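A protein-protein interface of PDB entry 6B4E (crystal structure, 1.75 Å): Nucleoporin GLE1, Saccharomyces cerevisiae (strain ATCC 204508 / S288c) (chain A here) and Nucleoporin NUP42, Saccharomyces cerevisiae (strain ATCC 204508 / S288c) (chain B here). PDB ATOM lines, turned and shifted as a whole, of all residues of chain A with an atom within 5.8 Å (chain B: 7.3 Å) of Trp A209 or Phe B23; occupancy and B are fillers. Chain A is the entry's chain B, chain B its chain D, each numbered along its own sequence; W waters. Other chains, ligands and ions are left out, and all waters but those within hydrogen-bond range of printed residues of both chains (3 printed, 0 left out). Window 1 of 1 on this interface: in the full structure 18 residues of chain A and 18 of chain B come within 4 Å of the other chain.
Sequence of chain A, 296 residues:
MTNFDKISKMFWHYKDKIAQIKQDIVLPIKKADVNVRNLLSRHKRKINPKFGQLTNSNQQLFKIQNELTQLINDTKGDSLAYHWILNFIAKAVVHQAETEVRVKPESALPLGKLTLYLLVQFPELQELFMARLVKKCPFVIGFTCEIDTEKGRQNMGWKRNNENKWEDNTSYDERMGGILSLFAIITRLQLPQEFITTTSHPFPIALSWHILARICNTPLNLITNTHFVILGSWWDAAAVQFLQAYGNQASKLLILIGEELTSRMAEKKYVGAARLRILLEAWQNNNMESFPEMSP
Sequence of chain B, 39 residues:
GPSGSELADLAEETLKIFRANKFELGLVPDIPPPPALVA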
ATOM      1  N   ILE A 205     -41.774 -25.637  20.419  1.00  0.00           N
ATOM      2  CA  ILE A 205     -40.534 -26.340  20.117  1.00  0.00           C
ATOM      3  C   ILE A 205     -39.411 -25.921  21.061  1.00  0.00           C
ATOM      4  O   ILE A 205     -38.482 -26.692  21.301  1.00  0.00           O
ATOM      5  CB  ILE A 205     -40.171 -26.135  18.626  1.00  0.00           C
ATOM      6  CG1 ILE A 205     -39.019 -27.043  18.199  1.00  0.00           C
ATOM      7  CG2 ILE A 205     -39.803 -24.681  18.302  1.00  0.00           C
ATOM      8  CD1 ILE A 205     -39.374 -28.479  18.164  1.00  0.00           C
ATOM      9  N   ALA A 206     -39.491 -24.711  21.635  1.00  0.00           N
ATOM     10  CA  ALA A 206     -38.516 -24.301  22.641  1.00  0.00           C
ATOM     11  C   ALA A 206     -38.387 -25.332  23.755  1.00  0.00           C
ATOM     12  O   ALA A 206     -37.319 -25.468  24.353  1.00  0.00           O
ATOM     13  CB  ALA A 206     -38.916 -22.944  23.242  1.00  0.00           C
ATOM     14  N   LEU A 207     -39.471 -26.042  24.070  1.00  0.00           N
ATOM     15  CA  LEU A 207     -39.424 -26.983  25.182  1.00  0.00           C
ATOM     16  C   LEU A 207     -38.562 -28.192  24.857  1.00  0.00           C
ATOM     17  O   LEU A 207     -38.012 -28.815  25.771  1.00  0.00           O
ATOM     18  CB  LEU A 207     -40.836 -27.417  25.560  1.00  0.00           C
ATOM     19  CG  LEU A 207     -41.782 -26.275  25.959  1.00  0.00           C
ATOM     20  CD1 LEU A 207     -43.056 -26.858  26.541  1.00  0.00           C
ATOM     21  CD2 LEU A 207     -41.130 -25.317  26.944  1.00  0.00           C
ATOM     22  N   SER A 208     -38.439 -28.540  23.567  1.00  0.00           N
ATOM     23  CA  SER A 208     -37.481 -29.554  23.148  1.00  0.00           C
ATOM     24  C   SER A 208     -36.056 -29.056  23.286  1.00  0.00           C
ATOM     25  O   SER A 208     -35.170 -29.831  23.659  1.00  0.00           O
ATOM     26  CB  SER A 208     -37.726 -29.988  21.698  1.00  0.00           C
ATOM     27  OG  SER A 208     -38.741 -30.970  21.615  1.00  0.00           O
ATOM     28  N   TRP A 209     -35.795 -27.784  22.953  1.00  0.00           N
ATOM     29  CA  TRP A 209     -34.475 -27.236  23.229  1.00  0.00           C
ATOM     30  C   TRP A 209     -34.135 -27.385  24.712  1.00  0.00           C
ATOM     31  O   TRP A 209     -33.043 -27.849  25.054  1.00  0.00           O
ATOM     32  CB  TRP A 209     -34.377 -25.765  22.789  1.00  0.00           C
ATOM     33  CG  TRP A 209     -32.994 -25.216  22.993  1.00  0.00           C
ATOM     34  CD1 TRP A 209     -32.466 -24.759  24.165  1.00  0.00           C
ATOM     35  CD2 TRP A 209     -31.958 -25.064  22.008  1.00  0.00           C
ATOM     36  NE1 TRP A 209     -31.177 -24.357  23.985  1.00  0.00           N
ATOM     37  CE2 TRP A 209     -30.831 -24.535  22.672  1.00  0.00           C
ATOM     38  CE3 TRP A 209     -31.870 -25.336  20.646  1.00  0.00           C
ATOM     39  CZ2 TRP A 209     -29.630 -24.275  22.023  1.00  0.00           C
ATOM     40  CZ3 TRP A 209     -30.672 -25.070  19.996  1.00  0.00           C
ATOM     41  CH2 TRP A 209     -29.569 -24.544  20.686  1.00  0.00           C
ATOM     42  N   HIS A 210     -35.091 -27.082  25.607  1.00  0.00           N
ATOM     43  CA  HIS A 210     -34.811 -27.159  27.043  1.00  0.00           C
ATOM     44  C   HIS A 210     -34.375 -28.559  27.447  1.00  0.00           C
ATOM     45  O   HIS A 210     -33.460 -28.725  28.264  1.00  0.00           O
ATOM     46  CB  HIS A 210     -36.038 -26.792  27.884  1.00  0.00           C
ATOM     47  CG  HIS A 210     -36.490 -25.373  27.750  1.00  0.00           C
ATOM     48  ND1 HIS A 210     -35.635 -24.339  27.433  1.00  0.00           N
ATOM     49  CD2 HIS A 210     -37.713 -24.816  27.911  1.00  0.00           C
ATOM     50  CE1 HIS A 210     -36.319 -23.207  27.378  1.00  0.00           C
ATOM     51  NE2 HIS A 210     -37.581 -23.466  27.677  1.00  0.00           N
ATOM     52  N   ILE A 211     -35.051 -29.580  26.922  1.00  0.00           N
ATOM     53  CA  ILE A 211     -34.738 -30.955  27.302  1.00  0.00           C
ATOM     54  C   ILE A 211     -33.302 -31.291  26.952  1.00  0.00           C
ATOM     55  O   ILE A 211     -32.552 -31.813  27.785  1.00  0.00           O
ATOM     56  CB  ILE A 211     -35.704 -31.939  26.622  1.00  0.00           C
ATOM     57  CG1 ILE A 211     -37.113 -31.749  27.172  1.00  0.00           C
ATOM     58  CG2 ILE A 211     -35.234 -33.392  26.844  1.00  0.00           C
ATOM     59  CD1 ILE A 211     -38.189 -32.479  26.387  1.00  0.00           C
ATOM     60  N   LEU A 212     -32.911 -31.032  25.698  1.00  0.00           N
ATOM     61  CA  LEU A 212     -31.577 -31.407  25.250  1.00  0.00           C
ATOM     62  C   LEU A 212     -30.517 -30.599  25.982  1.00  0.00           C
ATOM     63  O   LEU A 212     -29.495 -31.149  26.402  1.00  0.00           O
ATOM     64  CB  LEU A 212     -31.462 -31.217  23.732  1.00  0.00           C
ATOM     65  CG  LEU A 212     -31.904 -32.425  22.877  1.00  0.00           C
ATOM     66  CD1 LEU A 212     -33.367 -32.780  23.101  1.00  0.00           C
ATOM     67  CD2 LEU A 212     -31.639 -32.182  21.395  1.00  0.00           C
ATOM     68  N   ALA A 213     -30.737 -29.288  26.122  1.00  0.00           N
ATOM     69  CA  ALA A 213     -29.765 -28.439  26.798  1.00  0.00           C
ATOM     70  C   ALA A 213     -29.581 -28.857  28.246  1.00  0.00           C
ATOM     71  O   ALA A 213     -28.455 -28.897  28.746  1.00  0.00           O
ATOM     72  CB  ALA A 213     -30.202 -26.974  26.729  1.00  0.00           C
ATOM     73  N   ARG A 214     -30.682 -29.120  28.947  1.00  0.00           N
ATOM     74  CA  ARG A 214     -30.599 -29.405  30.376  1.00  0.00           C
ATOM     75  C   ARG A 214     -29.935 -30.746  30.643  1.00  0.00           C
ATOM     76  O   ARG A 214     -29.193 -30.892  31.624  1.00  0.00           O
ATOM     77  CB  ARG A 214     -31.996 -29.365  30.988  1.00  0.00           C
ATOM     78  CG  ARG A 214     -32.521 -27.930  31.044  1.00  0.00           C
ATOM     79  CD  ARG A 214     -33.995 -27.854  31.359  1.00  0.00           C
ATOM     80  NE  ARG A 214     -34.416 -26.462  31.300  1.00  0.00           N
ATOM     81  CZ  ARG A 214     -35.660 -26.027  31.429  1.00  0.00           C
ATOM     82  NH1 ARG A 214     -36.654 -26.864  31.679  1.00  0.00           N
ATOM     83  NH2 ARG A 214     -35.905 -24.731  31.298  1.00  0.00           N
ATOM     84  N   PHE A 242     -36.713 -30.227  14.632  1.00  0.00           N
ATOM     85  CA  PHE A 242     -35.802 -29.446  15.468  1.00  0.00           C
ATOM     86  C   PHE A 242     -34.755 -28.752  14.611  1.00  0.00           C
ATOM     87  O   PHE A 242     -34.459 -27.572  14.805  1.00  0.00           O
ATOM     88  CB  PHE A 242     -35.145 -30.387  16.480  1.00  0.00           C
ATOM     89  CG  PHE A 242     -34.368 -29.703  17.588  1.00  0.00           C
ATOM     90  CD1 PHE A 242     -35.017 -28.954  18.558  1.00  0.00           C
ATOM     91  CD2 PHE A 242     -33.001 -29.887  17.695  1.00  0.00           C
ATOM     92  CE1 PHE A 242     -34.308 -28.366  19.582  1.00  0.00           C
ATOM     93  CE2 PHE A 242     -32.285 -29.290  18.718  1.00  0.00           C
ATOM     94  CZ  PHE A 242     -32.944 -28.538  19.666  1.00  0.00           C
ATOM     95  N   TYR A 246     -34.153 -24.630  14.364  1.00  0.00           N
ATOM     96  CA  TYR A 246     -32.963 -23.963  14.886  1.00  0.00           C
ATOM     97  C   TYR A 246     -31.698 -24.194  14.065  1.00  0.00           C
ATOM     98  O   TYR A 246     -30.618 -23.768  14.501  1.00  0.00           O
ATOM     99  CB  TYR A 246     -32.720 -24.397  16.344  1.00  0.00           C
ATOM    100  CG  TYR A 246     -33.861 -24.103  17.294  1.00  0.00           C
ATOM    101  CD1 TYR A 246     -34.277 -22.817  17.539  1.00  0.00           C
ATOM    102  CD2 TYR A 246     -34.518 -25.141  17.974  1.00  0.00           C
ATOM    103  CE1 TYR A 246     -35.335 -22.550  18.420  1.00  0.00           C
ATOM    104  CE2 TYR A 246     -35.563 -24.877  18.851  1.00  0.00           C
ATOM    105  CZ  TYR A 246     -35.971 -23.587  19.068  1.00  0.00           C
ATOM    106  OH  TYR A 246     -37.009 -23.317  19.946  1.00  0.00           O
ATOM    107  N   GLN A 249     -27.748 -24.201  15.002  1.00  0.00           N
ATOM    108  CA  GLN A 249     -27.704 -24.310  16.457  1.00  0.00           C
ATOM    109  C   GLN A 249     -28.301 -25.628  16.919  1.00  0.00           C
ATOM    110  O   GLN A 249     -27.749 -26.299  17.801  1.00  0.00           O
ATOM    111  CB  GLN A 249     -28.421 -23.117  17.093  1.00  0.00           C
ATOM    112  CG  GLN A 249     -27.912 -21.764  16.596  1.00  0.00           C
ATOM    113  CD  GLN A 249     -26.495 -21.430  17.074  1.00  0.00           C
ATOM    114  OE1 GLN A 249     -25.878 -22.193  17.816  1.00  0.00           O
ATOM    115  NE2 GLN A 249     -25.982 -20.277  16.647  1.00  0.00           N
ATOM    116  N   ALA A 250     -29.408 -26.038  16.307  1.00  0.00           N
ATOM    117  CA  ALA A 250     -29.885 -27.401  16.511  1.00  0.00           C
ATOM    118  C   ALA A 250     -28.799 -28.407  16.182  1.00  0.00           C
ATOM    119  O   ALA A 250     -28.595 -29.371  16.927  1.00  0.00           O
ATOM    120  CB  ALA A 250     -31.106 -27.676  15.643  1.00  0.00           C
ATOM    121  N   LYS A 252     -25.509 -28.155  16.268  1.00  0.00           N
ATOM    122  CA  LYS A 252     -24.511 -28.219  17.332  1.00  0.00           C
ATOM    123  C   LYS A 252     -25.025 -29.032  18.513  1.00  0.00           C
ATOM    124  O   LYS A 252     -24.265 -29.772  19.148  1.00  0.00           O
ATOM    125  CB  LYS A 252     -24.136 -26.813  17.794  1.00  0.00           C
ATOM    126  CG  LYS A 252     -23.375 -26.022  16.736  1.00  0.00           C
ATOM    127  CD  LYS A 252     -23.495 -24.518  16.929  1.00  0.00           C
ATOM    128  CE  LYS A 252     -22.984 -24.067  18.274  1.00  0.00           C
ATOM    129  NZ  LYS A 252     -23.065 -22.571  18.414  1.00  0.00           N
ATOM    130  N   LEU A 253     -26.314 -28.905  18.832  1.00  0.00           N
ATOM    131  CA  LEU A 253     -26.832 -29.595  20.005  1.00  0.00           C
ATOM    132  C   LEU A 253     -27.032 -31.078  19.717  1.00  0.00           C
ATOM    133  O   LEU A 253     -26.823 -31.917  20.604  1.00  0.00           O
ATOM    134  CB  LEU A 253     -28.128 -28.912  20.462  1.00  0.00           C
ATOM    135  CG  LEU A 253     -28.721 -29.312  21.812  1.00  0.00           C
ATOM    136  CD1 LEU A 253     -27.661 -29.455  22.884  1.00  0.00           C
ATOM    137  CD2 LEU A 253     -29.746 -28.288  22.222  1.00  0.00           C
ATOM    138  N   LEU A 256     -23.748 -32.559  20.091  1.00  0.00           N
ATOM    139  CA  LEU A 256     -23.363 -32.651  21.491  1.00  0.00           C
ATOM    140  C   LEU A 256     -23.975 -33.887  22.137  1.00  0.00           C
ATOM    141  O   LEU A 256     -23.281 -34.627  22.840  1.00  0.00           O
ATOM    142  CB  LEU A 256     -23.757 -31.381  22.240  1.00  0.00           C
ATOM    143  CG  LEU A 256     -23.173 -31.267  23.652  1.00  0.00           C
ATOM    144  CD1 LEU A 256     -21.636 -31.128  23.630  1.00  0.00           C
ATOM    145  CD2 LEU A 256     -23.774 -30.094  24.341  1.00  0.00           C
ATOM    146  N   THR B  14     -22.893 -15.695  26.121  1.00  0.00           N
ATOM    147  CA  THR B  14     -23.859 -16.532  25.425  1.00  0.00           C
ATOM    148  C   THR B  14     -23.809 -16.292  23.923  1.00  0.00           C
ATOM    149  O   THR B  14     -23.910 -17.238  23.132  1.00  0.00           O
ATOM    150  CB  THR B  14     -25.258 -16.262  25.973  1.00  0.00           C
ATOM    151  OG1 THR B  14     -25.292 -16.603  27.363  1.00  0.00           O
ATOM    152  CG2 THR B  14     -26.297 -17.074  25.229  1.00  0.00           C
ATOM    153  N   ILE B  17     -20.993 -18.182  22.576  1.00  0.00           N
ATOM    154  CA  ILE B  17     -21.277 -19.610  22.503  1.00  0.00           C
ATOM    155  C   ILE B  17     -22.143 -19.928  21.293  1.00  0.00           C
ATOM    156  O   ILE B  17     -21.925 -20.933  20.603  1.00  0.00           O
ATOM    157  CB  ILE B  17     -21.928 -20.076  23.815  1.00  0.00           C
ATOM    158  CG1 ILE B  17     -20.890 -20.123  24.936  1.00  0.00           C
ATOM    159  CG2 ILE B  17     -22.530 -21.474  23.643  1.00  0.00           C
ATOM    160  CD1 ILE B  17     -21.496 -20.236  26.327  1.00  0.00           C
ATOM    161  N   PHE B  18     -23.130 -19.082  21.001  1.00  0.00           N
ATOM    162  CA  PHE B  18     -23.930 -19.310  19.806  1.00  0.00           C
ATOM    163  C   PHE B  18     -23.118 -19.083  18.535  1.00  0.00           C
ATOM    164  O   PHE B  18     -23.369 -19.752  17.526  1.00  0.00           O
ATOM    165  CB  PHE B  18     -25.171 -18.419  19.805  1.00  0.00           C
ATOM    166  CG  PHE B  18     -26.319 -18.965  20.629  1.00  0.00           C
ATOM    167  CD1 PHE B  18     -26.773 -20.275  20.452  1.00  0.00           C
ATOM    168  CD2 PHE B  18     -26.938 -18.176  21.588  1.00  0.00           C
ATOM    169  CE1 PHE B  18     -27.832 -20.762  21.206  1.00  0.00           C
ATOM    170  CE2 PHE B  18     -27.994 -18.662  22.343  1.00  0.00           C
ATOM    171  CZ  PHE B  18     -28.445 -19.958  22.149  1.00  0.00           C
ATOM    172  N   ARG B  19     -22.136 -18.173  18.553  1.00  0.00           N
ATOM    173  CA  ARG B  19     -21.274 -18.005  17.380  1.00  0.00           C
ATOM    174  C   ARG B  19     -20.311 -19.171  17.167  1.00  0.00           C
ATOM    175  O   ARG B  19     -19.820 -19.345  16.052  1.00  0.00           O
ATOM    176  CB  ARG B  19     -20.452 -16.718  17.472  1.00  0.00           C
ATOM    177  CG  ARG B  19     -21.249 -15.449  17.176  1.00  0.00           C
ATOM    178  CD  ARG B  19     -20.364 -14.241  16.951  1.00  0.00           C
ATOM    179  NE  ARG B  19     -19.538 -13.925  18.111  1.00  0.00           N
ATOM    180  CZ  ARG B  19     -19.881 -13.086  19.083  1.00  0.00           C
ATOM    181  NH1 ARG B  19     -21.055 -12.472  19.067  1.00  0.00           N
ATOM    182  NH2 ARG B  19     -19.044 -12.859  20.082  1.00  0.00           N
ATOM    183  N   ALA B  20     -20.006 -19.950  18.200  1.00  0.00           N
ATOM    184  CA  ALA B  20     -18.990 -20.984  18.075  1.00  0.00           C
ATOM    185  C   ALA B  20     -19.476 -22.117  17.174  1.00  0.00           C
ATOM    186  O   ALA B  20     -20.662 -22.258  16.898  1.00  0.00           O
ATOM    187  CB  ALA B  20     -18.628 -21.553  19.447  1.00  0.00           C
ATOM    188  N   ASN B  21     -18.535 -22.951  16.730  1.00  0.00           N
ATOM    189  CA  ASN B  21     -18.932 -24.113  15.944  1.00  0.00           C
ATOM    190  C   ASN B  21     -19.361 -25.292  16.810  1.00  0.00           C
ATOM    191  O   ASN B  21     -19.645 -26.368  16.271  1.00  0.00           O
ATOM    192  CB  ASN B  21     -17.801 -24.530  14.994  1.00  0.00           C
ATOM    193  CG  ASN B  21     -16.584 -25.067  15.703  1.00  0.00           C
ATOM    194  OD1 ASN B  21     -16.596 -25.331  16.903  1.00  0.00           O
ATOM    195  ND2 ASN B  21     -15.511 -25.244  14.947  1.00  0.00           N
ATOM    196  N   LYS B  22     -19.402 -25.139  18.130  1.00  0.00           N
ATOM    197  CA  LYS B  22     -19.811 -26.248  18.976  1.00  0.00           C
ATOM    198  C   LYS B  22     -20.334 -25.708  20.297  1.00  0.00           C
ATOM    199  O   LYS B  22     -20.027 -24.587  20.695  1.00  0.00           O
ATOM    200  CB  LYS B  22     -18.650 -27.220  19.226  1.00  0.00           C
ATOM    201  CG  LYS B  22     -17.537 -26.660  20.111  1.00  0.00           C
ATOM    202  CD  LYS B  22     -16.397 -27.650  20.349  1.00  0.00           C
ATOM    203  CE  LYS B  22     -15.365 -27.061  21.310  1.00  0.00           C
ATOM    204  NZ  LYS B  22     -14.288 -28.028  21.671  1.00  0.00           N
ATOM    205  N   PHE B  23     -21.138 -26.530  20.957  1.00  0.00           N
ATOM    206  CA  PHE B  23     -21.476 -26.370  22.361  1.00  0.00           C
ATOM    207  C   PHE B  23     -20.584 -27.289  23.194  1.00  0.00           C
ATOM    208  O   PHE B  23     -19.871 -28.154  22.674  1.00  0.00           O
ATOM    209  CB  PHE B  23     -22.950 -26.712  22.611  1.00  0.00           C
ATOM    210  CG  PHE B  23     -23.937 -25.774  21.955  1.00  0.00           C
ATOM    211  CD1 PHE B  23     -23.847 -24.403  22.121  1.00  0.00           C
ATOM    212  CD2 PHE B  23     -25.007 -26.299  21.221  1.00  0.00           C
ATOM    213  CE1 PHE B  23     -24.777 -23.556  21.538  1.00  0.00           C
ATOM    214  CE2 PHE B  23     -25.934 -25.461  20.637  1.00  0.00           C
ATOM    215  CZ  PHE B  23     -25.813 -24.083  20.798  1.00  0.00           C
ATOM    216  N   GLU B  24     -20.657 -27.112  24.509  1.00  0.00           N
ATOM    217  CA  GLU B  24     -19.958 -27.962  25.462  1.00  0.00           C
ATOM    218  C   GLU B  24     -20.895 -28.390  26.585  1.00  0.00           C
ATOM    219  O   GLU B  24     -21.777 -27.638  27.005  1.00  0.00           O
ATOM    220  CB  GLU B  24     -18.751 -27.233  26.043  1.00  0.00           C
ATOM    221  CG  GLU B  24     -17.639 -27.032  25.019  1.00  0.00           C
ATOM    222  CD  GLU B  24     -16.491 -26.271  25.581  1.00  0.00           C
ATOM    223  OE1 GLU B  24     -16.659 -25.056  25.790  1.00  0.00           O
ATOM    224  OE2 GLU B  24     -15.436 -26.891  25.829  1.00  0.00           O
ATOM    225  N   LEU B  25     -20.687 -29.613  27.075  1.00  0.00           N
ATOM    226  CA  LEU B  25     -21.470 -30.101  28.201  1.00  0.00           C
ATOM    227  C   LEU B  25     -21.322 -29.156  29.384  1.00  0.00           C
ATOM    228  O   LEU B  25     -20.218 -28.707  29.704  1.00  0.00           O
ATOM    229  CB  LEU B  25     -21.029 -31.513  28.594  1.00  0.00           C
ATOM    230  CG  LEU B  25     -21.144 -32.590  27.512  1.00  0.00           C
ATOM    231  CD1 LEU B  25     -20.552 -33.889  28.012  1.00  0.00           C
ATOM    232  CD2 LEU B  25     -22.594 -32.810  27.075  1.00  0.00           C
ATOM    233  N   GLY B  26     -22.447 -28.853  30.035  1.00  0.00           N
ATOM    234  CA  GLY B  26     -22.473 -27.941  31.161  1.00  0.00           C
ATOM    235  C   GLY B  26     -22.619 -26.483  30.789  1.00  0.00           C
ATOM    236  O   GLY B  26     -22.818 -25.646  31.688  1.00  0.00           O
ATOM    237  N   LEU B  27     -22.543 -26.151  29.497  1.00  0.00           N
ATOM    238  CA  LEU B  27     -22.511 -24.769  29.027  1.00  0.00           C
ATOM    239  C   LEU B  27     -23.481 -24.526  27.875  1.00  0.00           C
ATOM    240  O   LEU B  27     -23.346 -23.533  27.165  1.00  0.00           O
ATOM    241  CB  LEU B  27     -21.094 -24.391  28.589  1.00  0.00           C
ATOM    242  CG  LEU B  27     -20.045 -24.461  29.706  1.00  0.00           C
ATOM    243  CD1 LEU B  27     -18.655 -24.322  29.128  1.00  0.00           C
ATOM    244  CD2 LEU B  27     -20.298 -23.380  30.731  1.00  0.00           C
ATOM    245  N   VAL B  28     -24.435 -25.415  27.654  1.00  0.00           N
ATOM    246  CA  VAL B  28     -25.431 -25.161  26.606  1.00  0.00           C
ATOM    247  C   VAL B  28     -26.377 -24.060  27.075  1.00  0.00           C
ATOM    248  O   VAL B  28     -26.891 -24.136  28.200  1.00  0.00           O
ATOM    249  CB  VAL B  28     -26.211 -26.435  26.288  1.00  0.00           C
ATOM    250  CG1 VAL B  28     -27.119 -26.178  25.117  1.00  0.00           C
ATOM    251  CG2 VAL B  28     -25.275 -27.601  25.991  1.00  0.00           C
ATOM    252  N   PRO B  29     -26.657 -23.034  26.265  1.00  0.00           N
ATOM    253  CA  PRO B  29     -27.676 -22.058  26.668  1.00  0.00           C
ATOM    254  C   PRO B  29     -29.013 -22.744  26.922  1.00  0.00           C
ATOM    255  O   PRO B  29     -29.482 -23.544  26.107  1.00  0.00           O
ATOM    256  CB  PRO B  29     -27.741 -21.104  25.470  1.00  0.00           C
ATOM    257  CG  PRO B  29     -26.414 -21.222  24.823  1.00  0.00           C
ATOM    258  CD  PRO B  29     -26.080 -22.684  24.959  1.00  0.00           C
ATOM    259  N   ASP B  30     -29.612 -22.446  28.083  1.00  0.00           N
ATOM    260  CA  ASP B  30     -30.869 -23.092  28.453  1.00  0.00           C
ATOM    261  C   ASP B  30     -31.994 -22.667  27.524  1.00  0.00           C
ATOM    262  O   ASP B  30     -32.874 -23.473  27.195  1.00  0.00           O
ATOM    263  CB  ASP B  30     -31.224 -22.752  29.900  1.00  0.00           C
ATOM    264  CG  ASP B  30     -32.362 -23.603  30.458  1.00  0.00           C
ATOM    265  OD1 ASP B  30     -32.089 -24.720  30.948  1.00  0.00           O
ATOM    266  OD2 ASP B  30     -33.526 -23.139  30.463  1.00  0.00           O
ATOM    267  N   ILE B  31     -31.974 -21.408  27.099  1.00  0.00           N
ATOM    268  CA  ILE B  31     -32.998 -20.802  26.249  1.00  0.00           C
ATOM    269  C   ILE B  31     -32.576 -20.908  24.790  1.00  0.00           C
ATOM    270  O   ILE B  31     -31.418 -20.606  24.469  1.00  0.00           O
ATOM    271  CB  ILE B  31     -33.227 -19.335  26.646  1.00  0.00           C
ATOM    272  CG1 ILE B  31     -33.745 -19.286  28.086  1.00  0.00           C
ATOM    273  CG2 ILE B  31     -34.210 -18.657  25.691  1.00  0.00           C
ATOM    274  CD1 ILE B  31     -33.780 -17.902  28.674  1.00  0.00           C
ATOM    275  N   PRO B  32     -33.459 -21.311  23.878  1.00  0.00           N
ATOM    276  CA  PRO B  32     -33.048 -21.473  22.483  1.00  0.00           C
ATOM    277  C   PRO B  32     -32.680 -20.141  21.865  1.00  0.00           C
ATOM    278  O   PRO B  32     -33.121 -19.078  22.341  1.00  0.00           O
ATOM    279  CB  PRO B  32     -34.286 -22.073  21.805  1.00  0.00           C
ATOM    280  CG  PRO B  32     -35.433 -21.734  22.722  1.00  0.00           C
ATOM    281  CD  PRO B  32     -34.845 -21.769  24.095  1.00  0.00           C
ATOM    282  N   PRO B  33     -31.902 -20.171  20.783  1.00  0.00           N
ATOM    283  CA  PRO B  33     -31.509 -18.942  20.109  1.00  0.00           C
ATOM    284  C   PRO B  33     -32.682 -18.314  19.401  1.00  0.00           C
ATOM    285  O   PRO B  33     -33.578 -19.021  18.886  1.00  0.00           O
ATOM    286  CB  PRO B  33     -30.451 -19.413  19.098  1.00  0.00           C
ATOM    287  CG  PRO B  33     -30.910 -20.799  18.766  1.00  0.00           C
ATOM    288  CD  PRO B  33     -31.410 -21.366  20.074  1.00  0.00           C
ATOM    289  N   VAL B  38     -29.502 -17.865  14.208  1.00  0.00           N
ATOM    290  CA  VAL B  38     -29.503 -19.084  13.415  1.00  0.00           C
ATOM    291  C   VAL B  38     -29.030 -18.732  12.013  1.00  0.00           C
ATOM    292  O   VAL B  38     -29.562 -17.809  11.388  1.00  0.00           O
ATOM    293  CB  VAL B  38     -30.902 -19.722  13.391  1.00  0.00           C
ATOM    294  CG1 VAL B  38     -30.895 -20.978  12.508  1.00  0.00           C
ATOM    295  CG2 VAL B  38     -31.338 -20.064  14.815  1.00  0.00           C
HETATM  296  O   HOH W   1     -24.850 -17.028  16.240  1.00  0.00           O
HETATM  297  O   HOH W   2     -23.763 -19.191  14.454  1.00  0.00           O
HETATM  298  O   HOH W   3     -21.495 -29.249  19.459  1.00  0.00           O
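A ring nitrogen (ND1) of His A210 lies within hydrogen-bond range of the backbone carbonyl oxygen (O) of Asp B30. NE of Arg A214 lies within salt-bridge range of OD1 of Asp B30, at 2.9 Å. The backbone carbonyl oxygen (O) of Ile B17 lies within hydrogen-bond range of the side-chain amino group (NZ) of Lys A252, at 3.0 Å. The indole nitrogen (NE1) of Trp A209 is in hydrogen-bond range of the backbone carbonyl oxygen (O) of Pro B29 (2.8 Å). The backbone carbonyl oxygen of Phe B18 lies within hydrogen-bond range of the side-chain amino group of Lys A252 (3.0 Å). The side-chain amino group (NZ) of Lys A252 is in hydrogen-bond range of the backbone carbonyl oxygen (O) of Ala B20 (2.9 Å). NE2 of Gln A249 lies within hydrogen-bond range of O of Phe B18 (2.8 Å).
Phe B23 touches Trp A209 (CE2 to CH2, 3.7 Å). Trp A209 touches Asp B30. Trp A209 touches Ile B31 (NE1 to O, 3.8 Å). CD1 of Trp A209 touches N of Pro B32 (3.6 Å). Val B28 touches Ala A213 (CG1 to CB, 3.6 Å). Gln A249 touches Phe B23. Gln A249 touches Pro B33. Phe B23 touches Lys A252 (CD2 to CB, 3.6 Å). N of Leu A253 touches CD2 of Phe B23, at 3.8 Å. CG2 of Val B28 touches CD2 of Leu A256 (3.3 Å).
Hydrophobic or aromatic side chains of chain A within 4 Å of the printed part of chain B: Ala A206, Trp A209, His A210, Ala A213, Tyr A246 and Leu A256. Of the 19 printed residues of chain B, 14 touch a printed residue of chain A. Hydrophobic or aromatic side chains of chain B that line the printed part of chain A: Phe B18, Phe B23, Leu B25, Val B28, Pro B32, Pro B33 and Val B38. Among the printed residues, Asp or Glu carboxylates within 4 Å of a Lys or Arg side-chain nitrogen of the other chain: Arg A214 with Asp B30 (2.9 Å).
Water W3 bridges O of Lys A252 (2.8 Å) and N of Phe B23 (3.1 Å). Water W2 lies within hydrogen-bond range of the backbone carbonyl oxygen of Phe B18 and the side-chain amide nitrogen of Gln A249. Water W1 bridges O of Phe B18 (3.4 Å) and NE2 of Gln A249 (3.5 Å).
The side-chain amino group (NZ) of Lys A252 lies within hydrogen-bond range of the side-chain amide oxygen (OE1) of Gln A249 (2.9 Å). The backbone NH of Ala A206 sits close to the side-chain hydroxyl of Tyr A246 (3.3 Å).
Trp A209 touches six residues of chain B. Phe B23 touches five residues of chain A. Of the printed residues of chain B, Ala A206 touches Pro B32 (3.7 Å). Printed residues of chain B within 4 Å of Lys A252: Ile B17 (3.0 Å), Phe B18 (3.0 Å), Ala B20 (2.9 Å), Asn B21 (3.8 Å), Lys B22 (3.7 Å) and Phe B23 (3.6 Å). Ile A205 touches none of the printed residues of chain B. Leu B27 touches none of the printed residues of chain A. The nearest printed residue of chain B that does not touch Gln A249 is Val B38 (4.2 Å).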
